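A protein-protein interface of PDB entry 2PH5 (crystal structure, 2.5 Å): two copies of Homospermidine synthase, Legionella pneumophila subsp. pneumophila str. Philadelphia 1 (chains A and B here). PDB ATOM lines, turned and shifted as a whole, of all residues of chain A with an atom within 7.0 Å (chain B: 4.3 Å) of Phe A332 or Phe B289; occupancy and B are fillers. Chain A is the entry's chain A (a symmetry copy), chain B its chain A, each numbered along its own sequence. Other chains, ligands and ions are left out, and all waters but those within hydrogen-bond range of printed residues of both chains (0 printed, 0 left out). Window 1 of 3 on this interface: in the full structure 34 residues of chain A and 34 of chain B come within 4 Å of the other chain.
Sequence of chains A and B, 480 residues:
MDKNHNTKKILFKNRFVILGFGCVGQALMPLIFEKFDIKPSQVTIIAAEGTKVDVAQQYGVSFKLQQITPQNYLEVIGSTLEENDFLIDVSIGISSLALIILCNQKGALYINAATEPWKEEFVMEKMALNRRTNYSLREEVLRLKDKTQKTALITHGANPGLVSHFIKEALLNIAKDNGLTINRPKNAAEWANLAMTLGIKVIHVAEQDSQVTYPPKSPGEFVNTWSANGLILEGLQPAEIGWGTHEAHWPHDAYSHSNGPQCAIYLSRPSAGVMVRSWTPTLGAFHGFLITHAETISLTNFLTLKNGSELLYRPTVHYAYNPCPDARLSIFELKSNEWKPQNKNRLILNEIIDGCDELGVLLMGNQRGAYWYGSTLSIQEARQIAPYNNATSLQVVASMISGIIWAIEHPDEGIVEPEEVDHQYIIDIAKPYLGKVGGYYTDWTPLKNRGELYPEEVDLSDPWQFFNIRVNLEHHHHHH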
ATOM      1  N   PHE A 222     -24.030  23.231 -33.462  1.00  0.00           N
ATOM      2  CA  PHE A 222     -24.340  24.601 -33.092  1.00  0.00           C
ATOM      3  C   PHE A 222     -25.610  24.963 -33.871  1.00  0.00           C
ATOM      4  O   PHE A 222     -25.608  24.993 -35.104  1.00  0.00           O
ATOM      5  CB  PHE A 222     -23.179  25.529 -33.456  1.00  0.00           C
ATOM      6  CG  PHE A 222     -23.226  26.858 -32.755  1.00  0.00           C
ATOM      7  CD1 PHE A 222     -24.116  27.850 -33.168  1.00  0.00           C
ATOM      8  CD2 PHE A 222     -22.398  27.114 -31.658  1.00  0.00           C
ATOM      9  CE1 PHE A 222     -24.182  29.079 -32.502  1.00  0.00           C
ATOM     10  CE2 PHE A 222     -22.457  28.339 -30.986  1.00  0.00           C
ATOM     11  CZ  PHE A 222     -23.351  29.326 -31.408  1.00  0.00           C
ATOM     12  N   PHE A 289     -25.803  38.743 -24.232  1.00  0.00           N
ATOM     13  CA  PHE A 289     -24.375  38.598 -24.475  1.00  0.00           C
ATOM     14  C   PHE A 289     -23.919  39.886 -25.148  1.00  0.00           C
ATOM     15  O   PHE A 289     -24.612  40.409 -26.025  1.00  0.00           O
ATOM     16  CB  PHE A 289     -24.080  37.417 -25.418  1.00  0.00           C
ATOM     17  CG  PHE A 289     -24.326  36.071 -24.811  1.00  0.00           C
ATOM     18  CD1 PHE A 289     -25.599  35.505 -24.843  1.00  0.00           C
ATOM     19  CD2 PHE A 289     -23.296  35.385 -24.171  1.00  0.00           C
ATOM     20  CE1 PHE A 289     -25.850  34.273 -24.244  1.00  0.00           C
ATOM     21  CE2 PHE A 289     -23.533  34.154 -23.567  1.00  0.00           C
ATOM     22  CZ  PHE A 289     -24.816  33.594 -23.602  1.00  0.00           C
ATOM     23  N   ASP A 326     -31.864  27.537 -28.369  1.00  0.00           N
ATOM     24  CA  ASP A 326     -30.981  26.543 -28.971  1.00  0.00           C
ATOM     25  C   ASP A 326     -29.576  27.113 -29.151  1.00  0.00           C
ATOM     26  O   ASP A 326     -28.582  26.397 -28.986  1.00  0.00           O
ATOM     27  CB  ASP A 326     -31.526  26.077 -30.325  1.00  0.00           C
ATOM     28  CG  ASP A 326     -32.621  25.029 -30.192  1.00  0.00           C
ATOM     29  OD1 ASP A 326     -33.275  24.728 -31.212  1.00  0.00           O
ATOM     30  OD2 ASP A 326     -32.823  24.497 -29.080  1.00  0.00           O
ATOM     31  N   ALA A 327     -29.494  28.397 -29.496  1.00  0.00           N
ATOM     32  CA  ALA A 327     -28.196  29.039 -29.670  1.00  0.00           C
ATOM     33  C   ALA A 327     -27.572  29.268 -28.289  1.00  0.00           C
ATOM     34  O   ALA A 327     -26.357  29.398 -28.167  1.00  0.00           O
ATOM     35  CB  ALA A 327     -28.346  30.366 -30.410  1.00  0.00           C
ATOM     36  N   ARG A 328     -28.406  29.313 -27.252  1.00  0.00           N
ATOM     37  CA  ARG A 328     -27.914  29.502 -25.889  1.00  0.00           C
ATOM     38  C   ARG A 328     -27.239  28.219 -25.467  1.00  0.00           C
ATOM     39  O   ARG A 328     -26.136  28.231 -24.914  1.00  0.00           O
ATOM     40  CB  ARG A 328     -29.057  29.811 -24.931  1.00  0.00           C
ATOM     41  CG  ARG A 328     -29.771  31.096 -25.251  1.00  0.00           C
ATOM     42  CD  ARG A 328     -31.066  31.235 -24.448  1.00  0.00           C
ATOM     43  NE  ARG A 328     -31.986  32.121 -25.145  1.00  0.00           N
ATOM     44  CZ  ARG A 328     -33.265  32.281 -24.835  1.00  0.00           C
ATOM     45  NH1 ARG A 328     -34.011  33.116 -25.553  1.00  0.00           N
ATOM     46  NH2 ARG A 328     -33.788  31.613 -23.812  1.00  0.00           N
ATOM     47  N   LEU A 329     -27.909  27.109 -25.744  1.00  0.00           N
ATOM     48  CA  LEU A 329     -27.371  25.799 -25.426  1.00  0.00           C
ATOM     49  C   LEU A 329     -26.105  25.602 -26.256  1.00  0.00           C
ATOM     50  O   LEU A 329     -25.134  25.015 -25.786  1.00  0.00           O
ATOM     51  CB  LEU A 329     -28.390  24.702 -25.769  1.00  0.00           C
ATOM     52  CG  LEU A 329     -29.706  24.673 -24.991  1.00  0.00           C
ATOM     53  CD1 LEU A 329     -30.646  23.622 -25.580  1.00  0.00           C
ATOM     54  CD2 LEU A 329     -29.436  24.363 -23.534  1.00  0.00           C
ATOM     55  N   SER A 330     -26.117  26.101 -27.490  1.00  0.00           N
ATOM     56  CA  SER A 330     -24.961  25.961 -28.370  1.00  0.00           C
ATOM     57  C   SER A 330     -23.731  26.671 -27.826  1.00  0.00           C
ATOM     58  O   SER A 330     -22.647  26.090 -27.753  1.00  0.00           O
ATOM     59  CB  SER A 330     -25.291  26.485 -29.770  1.00  0.00           C
ATOM     60  OG  SER A 330     -26.221  25.637 -30.418  1.00  0.00           O
ATOM     61  N   ILE A 331     -23.899  27.933 -27.455  1.00  0.00           N
ATOM     62  CA  ILE A 331     -22.805  28.710 -26.886  1.00  0.00           C
ATOM     63  C   ILE A 331     -22.299  28.004 -25.619  1.00  0.00           C
ATOM     64  O   ILE A 331     -21.090  27.874 -25.415  1.00  0.00           O
ATOM     65  CB  ILE A 331     -23.285  30.137 -26.557  1.00  0.00           C
ATOM     66  CG1 ILE A 331     -23.488  30.912 -27.867  1.00  0.00           C
ATOM     67  CG2 ILE A 331     -22.298  30.833 -25.633  1.00  0.00           C
ATOM     68  CD1 ILE A 331     -24.274  32.196 -27.714  1.00  0.00           C
ATOM     69  N   PHE A 332     -23.225  27.540 -24.782  1.00  0.00           N
ATOM     70  CA  PHE A 332     -22.863  26.833 -23.554  1.00  0.00           C
ATOM     71  C   PHE A 332     -21.957  25.643 -23.890  1.00  0.00           C
ATOM     72  O   PHE A 332     -20.912  25.450 -23.257  1.00  0.00           O
ATOM     73  CB  PHE A 332     -24.135  26.374 -22.822  1.00  0.00           C
ATOM     74  CG  PHE A 332     -23.877  25.548 -21.584  1.00  0.00           C
ATOM     75  CD1 PHE A 332     -23.679  24.169 -21.676  1.00  0.00           C
ATOM     76  CD2 PHE A 332     -23.850  26.146 -20.322  1.00  0.00           C
ATOM     77  CE1 PHE A 332     -23.460  23.393 -20.531  1.00  0.00           C
ATOM     78  CE2 PHE A 332     -23.631  25.375 -19.171  1.00  0.00           C
ATOM     79  CZ  PHE A 332     -23.436  23.997 -19.280  1.00  0.00           C
ATOM     80  N   GLU A 333     -22.352  24.866 -24.898  1.00  0.00           N
ATOM     81  CA  GLU A 333     -21.592  23.698 -25.338  1.00  0.00           C
ATOM     82  C   GLU A 333     -20.244  24.103 -25.954  1.00  0.00           C
ATOM     83  O   GLU A 333     -19.256  23.380 -25.818  1.00  0.00           O
ATOM     84  CB  GLU A 333     -22.434  22.890 -26.341  1.00  0.00           C
ATOM     85  CG  GLU A 333     -21.728  21.727 -27.025  1.00  0.00           C
ATOM     86  CD  GLU A 333     -22.663  20.928 -27.939  1.00  0.00           C
ATOM     87  OE1 GLU A 333     -23.338  21.540 -28.800  1.00  0.00           O
ATOM     88  OE2 GLU A 333     -22.725  19.679 -27.800  1.00  0.00           O
ATOM     89  N   LEU A 334     -20.218  25.265 -26.611  1.00  0.00           N
ATOM     90  CA  LEU A 334     -19.019  25.818 -27.251  1.00  0.00           C
ATOM     91  C   LEU A 334     -17.954  26.060 -26.188  1.00  0.00           C
ATOM     92  O   LEU A 334     -16.820  25.602 -26.313  1.00  0.00           O
ATOM     93  CB  LEU A 334     -19.354  27.151 -27.929  1.00  0.00           C
ATOM     94  CG  LEU A 334     -18.487  27.753 -29.049  1.00  0.00           C
ATOM     95  CD1 LEU A 334     -18.384  29.255 -28.807  1.00  0.00           C
ATOM     96  CD2 LEU A 334     -17.114  27.126 -29.124  1.00  0.00           C
ATOM     97  N   LYS A 335     -18.331  26.794 -25.141  1.00  0.00           N
ATOM     98  CA  LYS A 335     -17.422  27.091 -24.038  1.00  0.00           C
ATOM     99  C   LYS A 335     -17.024  25.777 -23.381  1.00  0.00           C
ATOM    100  O   LYS A 335     -15.865  25.584 -23.014  1.00  0.00           O
ATOM    101  CB  LYS A 335     -18.102  27.982 -22.993  1.00  0.00           C
ATOM    102  CG  LYS A 335     -18.500  29.351 -23.490  1.00  0.00           C
ATOM    103  CD  LYS A 335     -19.333  30.081 -22.461  1.00  0.00           C
ATOM    104  CE  LYS A 335     -19.663  31.473 -22.965  1.00  0.00           C
ATOM    105  NZ  LYS A 335     -20.516  32.266 -22.032  1.00  0.00           N
ATOM    106  N   SER A 336     -18.003  24.886 -23.231  1.00  0.00           N
ATOM    107  CA  SER A 336     -17.789  23.571 -22.637  1.00  0.00           C
ATOM    108  C   SER A 336     -16.721  22.798 -23.415  1.00  0.00           C
ATOM    109  O   SER A 336     -15.991  21.990 -22.844  1.00  0.00           O
ATOM    110  CB  SER A 336     -19.105  22.784 -22.631  1.00  0.00           C
ATOM    111  OG  SER A 336     -18.935  21.473 -22.119  1.00  0.00           O
ATOM    112  N   ASN A 337     -16.637  23.052 -24.721  1.00  0.00           N
ATOM    113  CA  ASN A 337     -15.651  22.396 -25.572  1.00  0.00           C
ATOM    114  C   ASN A 337     -14.403  23.257 -25.689  1.00  0.00           C
ATOM    115  O   ASN A 337     -13.717  23.232 -26.715  1.00  0.00           O
ATOM    116  CB  ASN A 337     -16.186  22.164 -26.988  1.00  0.00           C
ATOM    117  CG  ASN A 337     -17.422  21.302 -27.021  1.00  0.00           C
ATOM    118  OD1 ASN A 337     -17.556  20.338 -26.265  1.00  0.00           O
ATOM    119  ND2 ASN A 337     -18.335  21.633 -27.926  1.00  0.00           N
ATOM    120  N   GLN A 342     -18.353  23.212 -32.515  1.00  0.00           N
ATOM    121  CA  GLN A 342     -18.929  21.899 -32.789  1.00  0.00           C
ATOM    122  C   GLN A 342     -18.605  21.505 -34.226  1.00  0.00           C
ATOM    123  O   GLN A 342     -18.509  22.361 -35.102  1.00  0.00           O
ATOM    124  CB  GLN A 342     -20.452  21.938 -32.616  1.00  0.00           C
ATOM    125  CG  GLN A 342     -20.970  22.128 -31.192  1.00  0.00           C
ATOM    126  CD  GLN A 342     -21.257  23.578 -30.829  1.00  0.00           C
ATOM    127  OE1 GLN A 342     -22.184  23.861 -30.065  1.00  0.00           O
ATOM    128  NE2 GLN A 342     -20.459  24.502 -31.358  1.00  0.00           N
ATOM    129  N   ALA B 272     -23.758  27.687  -8.692  1.00  0.00           N
ATOM    130  CA  ALA B 272     -24.251  27.735 -10.065  1.00  0.00           C
ATOM    131  C   ALA B 272     -23.423  28.712 -10.914  1.00  0.00           C
ATOM    132  O   ALA B 272     -23.609  28.813 -12.130  1.00  0.00           O
ATOM    133  CB  ALA B 272     -25.724  28.149 -10.079  1.00  0.00           C
ATOM    134  N   VAL B 274     -19.995  28.656 -10.772  1.00  0.00           N
ATOM    135  CA  VAL B 274     -18.675  28.042 -10.854  1.00  0.00           C
ATOM    136  C   VAL B 274     -18.738  26.807 -11.759  1.00  0.00           C
ATOM    137  O   VAL B 274     -19.562  25.916 -11.550  1.00  0.00           O
ATOM    138  CB  VAL B 274     -18.178  27.568  -9.461  1.00  0.00           C
ATOM    139  CG1 VAL B 274     -16.718  27.154  -9.542  1.00  0.00           C
ATOM    140  CG2 VAL B 274     -18.374  28.665  -8.421  1.00  0.00           C
ATOM    141  N   MET B 275     -17.873  26.750 -12.764  1.00  0.00           N
ATOM    142  CA  MET B 275     -17.836  25.614 -13.674  1.00  0.00           C
ATOM    143  C   MET B 275     -16.559  24.805 -13.428  1.00  0.00           C
ATOM    144  O   MET B 275     -15.506  25.357 -13.098  1.00  0.00           O
ATOM    145  CB  MET B 275     -17.845  26.099 -15.128  1.00  0.00           C
ATOM    146  CG  MET B 275     -18.985  27.030 -15.500  1.00  0.00           C
ATOM    147  SD  MET B 275     -20.730  26.244 -15.240  1.00  0.00           S
ATOM    148  CE  MET B 275     -20.711  24.949 -16.688  1.00  0.00           C
ATOM    149  N   HIS B 287     -18.238  20.748 -19.225  1.00  0.00           N
ATOM    150  CA  HIS B 287     -18.126  21.714 -18.142  1.00  0.00           C
ATOM    151  C   HIS B 287     -19.386  21.646 -17.292  1.00  0.00           C
ATOM    152  O   HIS B 287     -20.456  22.087 -17.712  1.00  0.00           O
ATOM    153  CB  HIS B 287     -17.956  23.140 -18.669  1.00  0.00           C
ATOM    154  CG  HIS B 287     -16.603  23.418 -19.249  1.00  0.00           C
ATOM    155  ND1 HIS B 287     -16.167  24.693 -19.541  1.00  0.00           N
ATOM    156  CD2 HIS B 287     -15.600  22.583 -19.613  1.00  0.00           C
ATOM    157  CE1 HIS B 287     -14.953  24.631 -20.059  1.00  0.00           C
ATOM    158  NE2 HIS B 287     -14.586  23.362 -20.114  1.00  0.00           N
ATOM    159  N   GLY B 288     -19.262  21.096 -16.092  1.00  0.00           N
ATOM    160  CA  GLY B 288     -20.422  21.008 -15.223  1.00  0.00           C
ATOM    161  C   GLY B 288     -20.456  22.106 -14.171  1.00  0.00           C
ATOM    162  O   GLY B 288     -19.441  22.753 -13.908  1.00  0.00           O
ATOM    163  N   PHE B 289     -21.627  22.334 -13.584  1.00  0.00           N
ATOM    164  CA  PHE B 289     -21.773  23.330 -12.532  1.00  0.00           C
ATOM    165  C   PHE B 289     -21.265  22.684 -11.251  1.00  0.00           C
ATOM    166  O   PHE B 289     -21.549  21.510 -10.992  1.00  0.00           O
ATOM    167  CB  PHE B 289     -23.247  23.730 -12.332  1.00  0.00           C
ATOM    168  CG  PHE B 289     -23.824  24.529 -13.459  1.00  0.00           C
ATOM    169  CD1 PHE B 289     -24.367  23.890 -14.572  1.00  0.00           C
ATOM    170  CD2 PHE B 289     -23.790  25.921 -13.428  1.00  0.00           C
ATOM    171  CE1 PHE B 289     -24.868  24.623 -15.645  1.00  0.00           C
ATOM    172  CE2 PHE B 289     -24.286  26.667 -14.493  1.00  0.00           C
ATOM    173  CZ  PHE B 289     -24.827  26.016 -15.609  1.00  0.00           C
ATOM    174  N   LEU B 290     -20.512  23.439 -10.458  1.00  0.00           N
ATOM    175  CA  LEU B 290     -19.983  22.924  -9.199  1.00  0.00           C
ATOM    176  C   LEU B 290     -21.031  23.089  -8.093  1.00  0.00           C
ATOM    177  O   LEU B 290     -20.778  23.702  -7.056  1.00  0.00           O
ATOM    178  CB  LEU B 290     -18.679  23.653  -8.851  1.00  0.00           C
ATOM    179  CG  LEU B 290     -17.842  23.331  -7.596  1.00  0.00           C
ATOM    180  CD1 LEU B 290     -17.958  21.893  -7.166  1.00  0.00           C
ATOM    181  CD2 LEU B 290     -16.394  23.690  -7.902  1.00  0.00           C
ATOM    182  N   ILE B 291     -22.215  22.537  -8.356  1.00  0.00           N
ATOM    183  CA  ILE B 291     -23.343  22.559  -7.435  1.00  0.00           C
ATOM    184  C   ILE B 291     -22.956  21.886  -6.132  1.00  0.00           C
ATOM    185  O   ILE B 291     -22.399  20.797  -6.128  1.00  0.00           O
ATOM    186  CB  ILE B 291     -24.574  21.815  -8.030  1.00  0.00           C
ATOM    187  CG1 ILE B 291     -25.580  22.815  -8.595  1.00  0.00           C
ATOM    188  CG2 ILE B 291     -25.284  21.009  -6.959  1.00  0.00           C
ATOM    189  CD1 ILE B 291     -25.049  23.659  -9.687  1.00  0.00           C
ATOM    190  N   TYR B 319     -18.919  18.136  -6.667  1.00  0.00           N
ATOM    191  CA  TYR B 319     -19.891  17.793  -7.697  1.00  0.00           C
ATOM    192  C   TYR B 319     -19.616  18.550  -9.017  1.00  0.00           C
ATOM    193  O   TYR B 319     -19.245  19.722  -9.004  1.00  0.00           O
ATOM    194  CB  TYR B 319     -21.290  18.136  -7.136  1.00  0.00           C
ATOM    195  CG  TYR B 319     -22.497  17.519  -7.826  1.00  0.00           C
ATOM    196  CD1 TYR B 319     -23.796  17.967  -7.537  1.00  0.00           C
ATOM    197  CD2 TYR B 319     -22.348  16.499  -8.770  1.00  0.00           C
ATOM    198  CE1 TYR B 319     -24.919  17.411  -8.181  1.00  0.00           C
ATOM    199  CE2 TYR B 319     -23.451  15.936  -9.415  1.00  0.00           C
ATOM    200  CZ  TYR B 319     -24.731  16.396  -9.115  1.00  0.00           C
ATOM    201  OH  TYR B 319     -25.817  15.827  -9.750  1.00  0.00           O
ATOM    202  N   ALA B 320     -19.773  17.859 -10.146  1.00  0.00           N
ATOM    203  CA  ALA B 320     -19.592  18.429 -11.491  1.00  0.00           C
ATOM    204  C   ALA B 320     -20.886  18.066 -12.224  1.00  0.00           C
ATOM    205  O   ALA B 320     -20.962  17.046 -12.918  1.00  0.00           O
ATOM    206  CB  ALA B 320     -18.385  17.782 -12.189  1.00  0.00           C
ATOM    207  N   TYR B 321     -21.900  18.906 -12.056  1.00  0.00           N
ATOM    208  CA  TYR B 321     -23.229  18.673 -12.619  1.00  0.00           C
ATOM    209  C   TYR B 321     -23.573  19.420 -13.894  1.00  0.00           C
ATOM    210  O   TYR B 321     -23.276  20.602 -14.045  1.00  0.00           O
ATOM    211  CB  TYR B 321     -24.285  19.028 -11.566  1.00  0.00           C
ATOM    212  CG  TYR B 321     -25.724  18.705 -11.936  1.00  0.00           C
ATOM    213  CD1 TYR B 321     -26.758  19.572 -11.589  1.00  0.00           C
ATOM    214  CD2 TYR B 321     -26.063  17.497 -12.558  1.00  0.00           C
ATOM    215  CE1 TYR B 321     -28.086  19.248 -11.838  1.00  0.00           C
ATOM    216  CE2 TYR B 321     -27.401  17.163 -12.811  1.00  0.00           C
ATOM    217  CZ  TYR B 321     -28.405  18.044 -12.445  1.00  0.00           C
ATOM    218  OH  TYR B 321     -29.724  17.719 -12.674  1.00  0.00           O
ATOM    219  N   ASN B 322     -24.231  18.714 -14.801  1.00  0.00           N
ATOM    220  CA  ASN B 322     -24.681  19.302 -16.050  1.00  0.00           C
ATOM    221  C   ASN B 322     -26.109  18.794 -16.183  1.00  0.00           C
ATOM    222  O   ASN B 322     -26.337  17.651 -16.594  1.00  0.00           O
ATOM    223  CB  ASN B 322     -23.833  18.818 -17.220  1.00  0.00           C
ATOM    224  CG  ASN B 322     -24.119  19.582 -18.496  1.00  0.00           C
ATOM    225  OD1 ASN B 322     -23.671  19.199 -19.573  1.00  0.00           O
ATOM    226  ND2 ASN B 322     -24.860  20.673 -18.382  1.00  0.00           N
ATOM    227  N   PRO B 323     -27.090  19.635 -15.812  1.00  0.00           N
ATOM    228  CA  PRO B 323     -28.517  19.302 -15.866  1.00  0.00           C
ATOM    229  C   PRO B 323     -29.051  19.172 -17.288  1.00  0.00           C
ATOM    230  O   PRO B 323     -28.321  19.365 -18.261  1.00  0.00           O
ATOM    231  CB  PRO B 323     -29.160  20.456 -15.109  1.00  0.00           C
ATOM    232  CG  PRO B 323     -28.312  21.606 -15.527  1.00  0.00           C
ATOM    233  CD  PRO B 323     -26.901  21.047 -15.426  1.00  0.00           C
ATOM    234  N   ILE B 331     -31.477  27.870 -15.373  1.00  0.00           N
ATOM    235  CA  ILE B 331     -30.430  28.516 -14.591  1.00  0.00           C
ATOM    236  C   ILE B 331     -30.026  29.826 -15.283  1.00  0.00           C
ATOM    237  O   ILE B 331     -29.873  30.859 -14.629  1.00  0.00           O
ATOM    238  CB  ILE B 331     -29.215  27.576 -14.457  1.00  0.00           C
ATOM    239  CG1 ILE B 331     -29.573  26.429 -13.500  1.00  0.00           C
ATOM    240  CG2 ILE B 331     -27.992  28.346 -13.986  1.00  0.00           C
ATOM    241  CD1 ILE B 331     -28.609  25.262 -13.542  1.00  0.00           C
ATOM    242  N   LYS B 335     -30.223  33.538 -13.383  1.00  0.00           N
ATOM    243  CA  LYS B 335     -29.172  34.543 -13.250  1.00  0.00           C
ATOM    244  C   LYS B 335     -29.635  35.813 -13.948  1.00  0.00           C
ATOM    245  O   LYS B 335     -29.419  36.918 -13.449  1.00  0.00           O
ATOM    246  CB  LYS B 335     -27.871  34.064 -13.904  1.00  0.00           C
ATOM    247  CG  LYS B 335     -27.258  32.837 -13.271  1.00  0.00           C
ATOM    248  CD  LYS B 335     -26.098  32.324 -14.094  1.00  0.00           C
ATOM    249  CE  LYS B 335     -25.468  31.132 -13.401  1.00  0.00           C
ATOM    250  NZ  LYS B 335     -24.329  30.527 -14.154  1.00  0.00           N
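The backbone NH (N) of His B287 is in hydrogen-bond range of the side-chain hydroxyl (OG) of Ser A336, at 3.1 Å.
Hydrophobic or aromatic side chains of chain A within 4 Å of the printed part of chain B: Phe A332. Along chain A the printed residues that touch a printed residue of chain B span positions 332 to 336. Among the printed residues, no Asp or Glu carboxylate lies within 4 Å of a Lys or Arg side-chain nitrogen of the other chain.
O of Tyr B321 is in hydrogen-bond range of N of Phe B289 (2.4 Å).
Among the printed residues, pairs that only touch across the chains: Lys A335 with His B287 (3.2 Å), Phe A332 with Asn B322 (3.7 Å), Phe A332 with Phe B289 (3.8 Å), Phe A332 with Met B275 (3.9 Å) and Phe A332 with His B287 (3.9 Å).
Phe A332 touches four residues of chain B. Of the printed residues of chain B, Lys A335 touches His B287. Of the printed residues of chain B, Ser A336 touches His B287 (3.1 Å). Val B274 touches none of the printed residues of chain A. Printed residues of chain A within 4 Å of Met B275: Phe A332 (3.9 Å). Of the printed residues of chain A, His B287 touches Phe A332, Lys A335 and Ser A336. Of chain A, only Phe A332 (3.8 Å) comes within 4 Å of Phe B289. Ile B291 touches none of the printed residues of chain A. Printed residues of chain A within 4 Å of Asn B322: Phe A332. The nearest printed residue of chain B that does not touch Phe A332 is Gly B288 (5.9 Å). The nearest printed residue of chain A that does not touch His B287 is Asn A337 (5.1 Å).
3 positions are printed for both chains. Of the 6 pairs that touch across the chains among the printed residues, none has its exchanged pair printed and touching as well.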
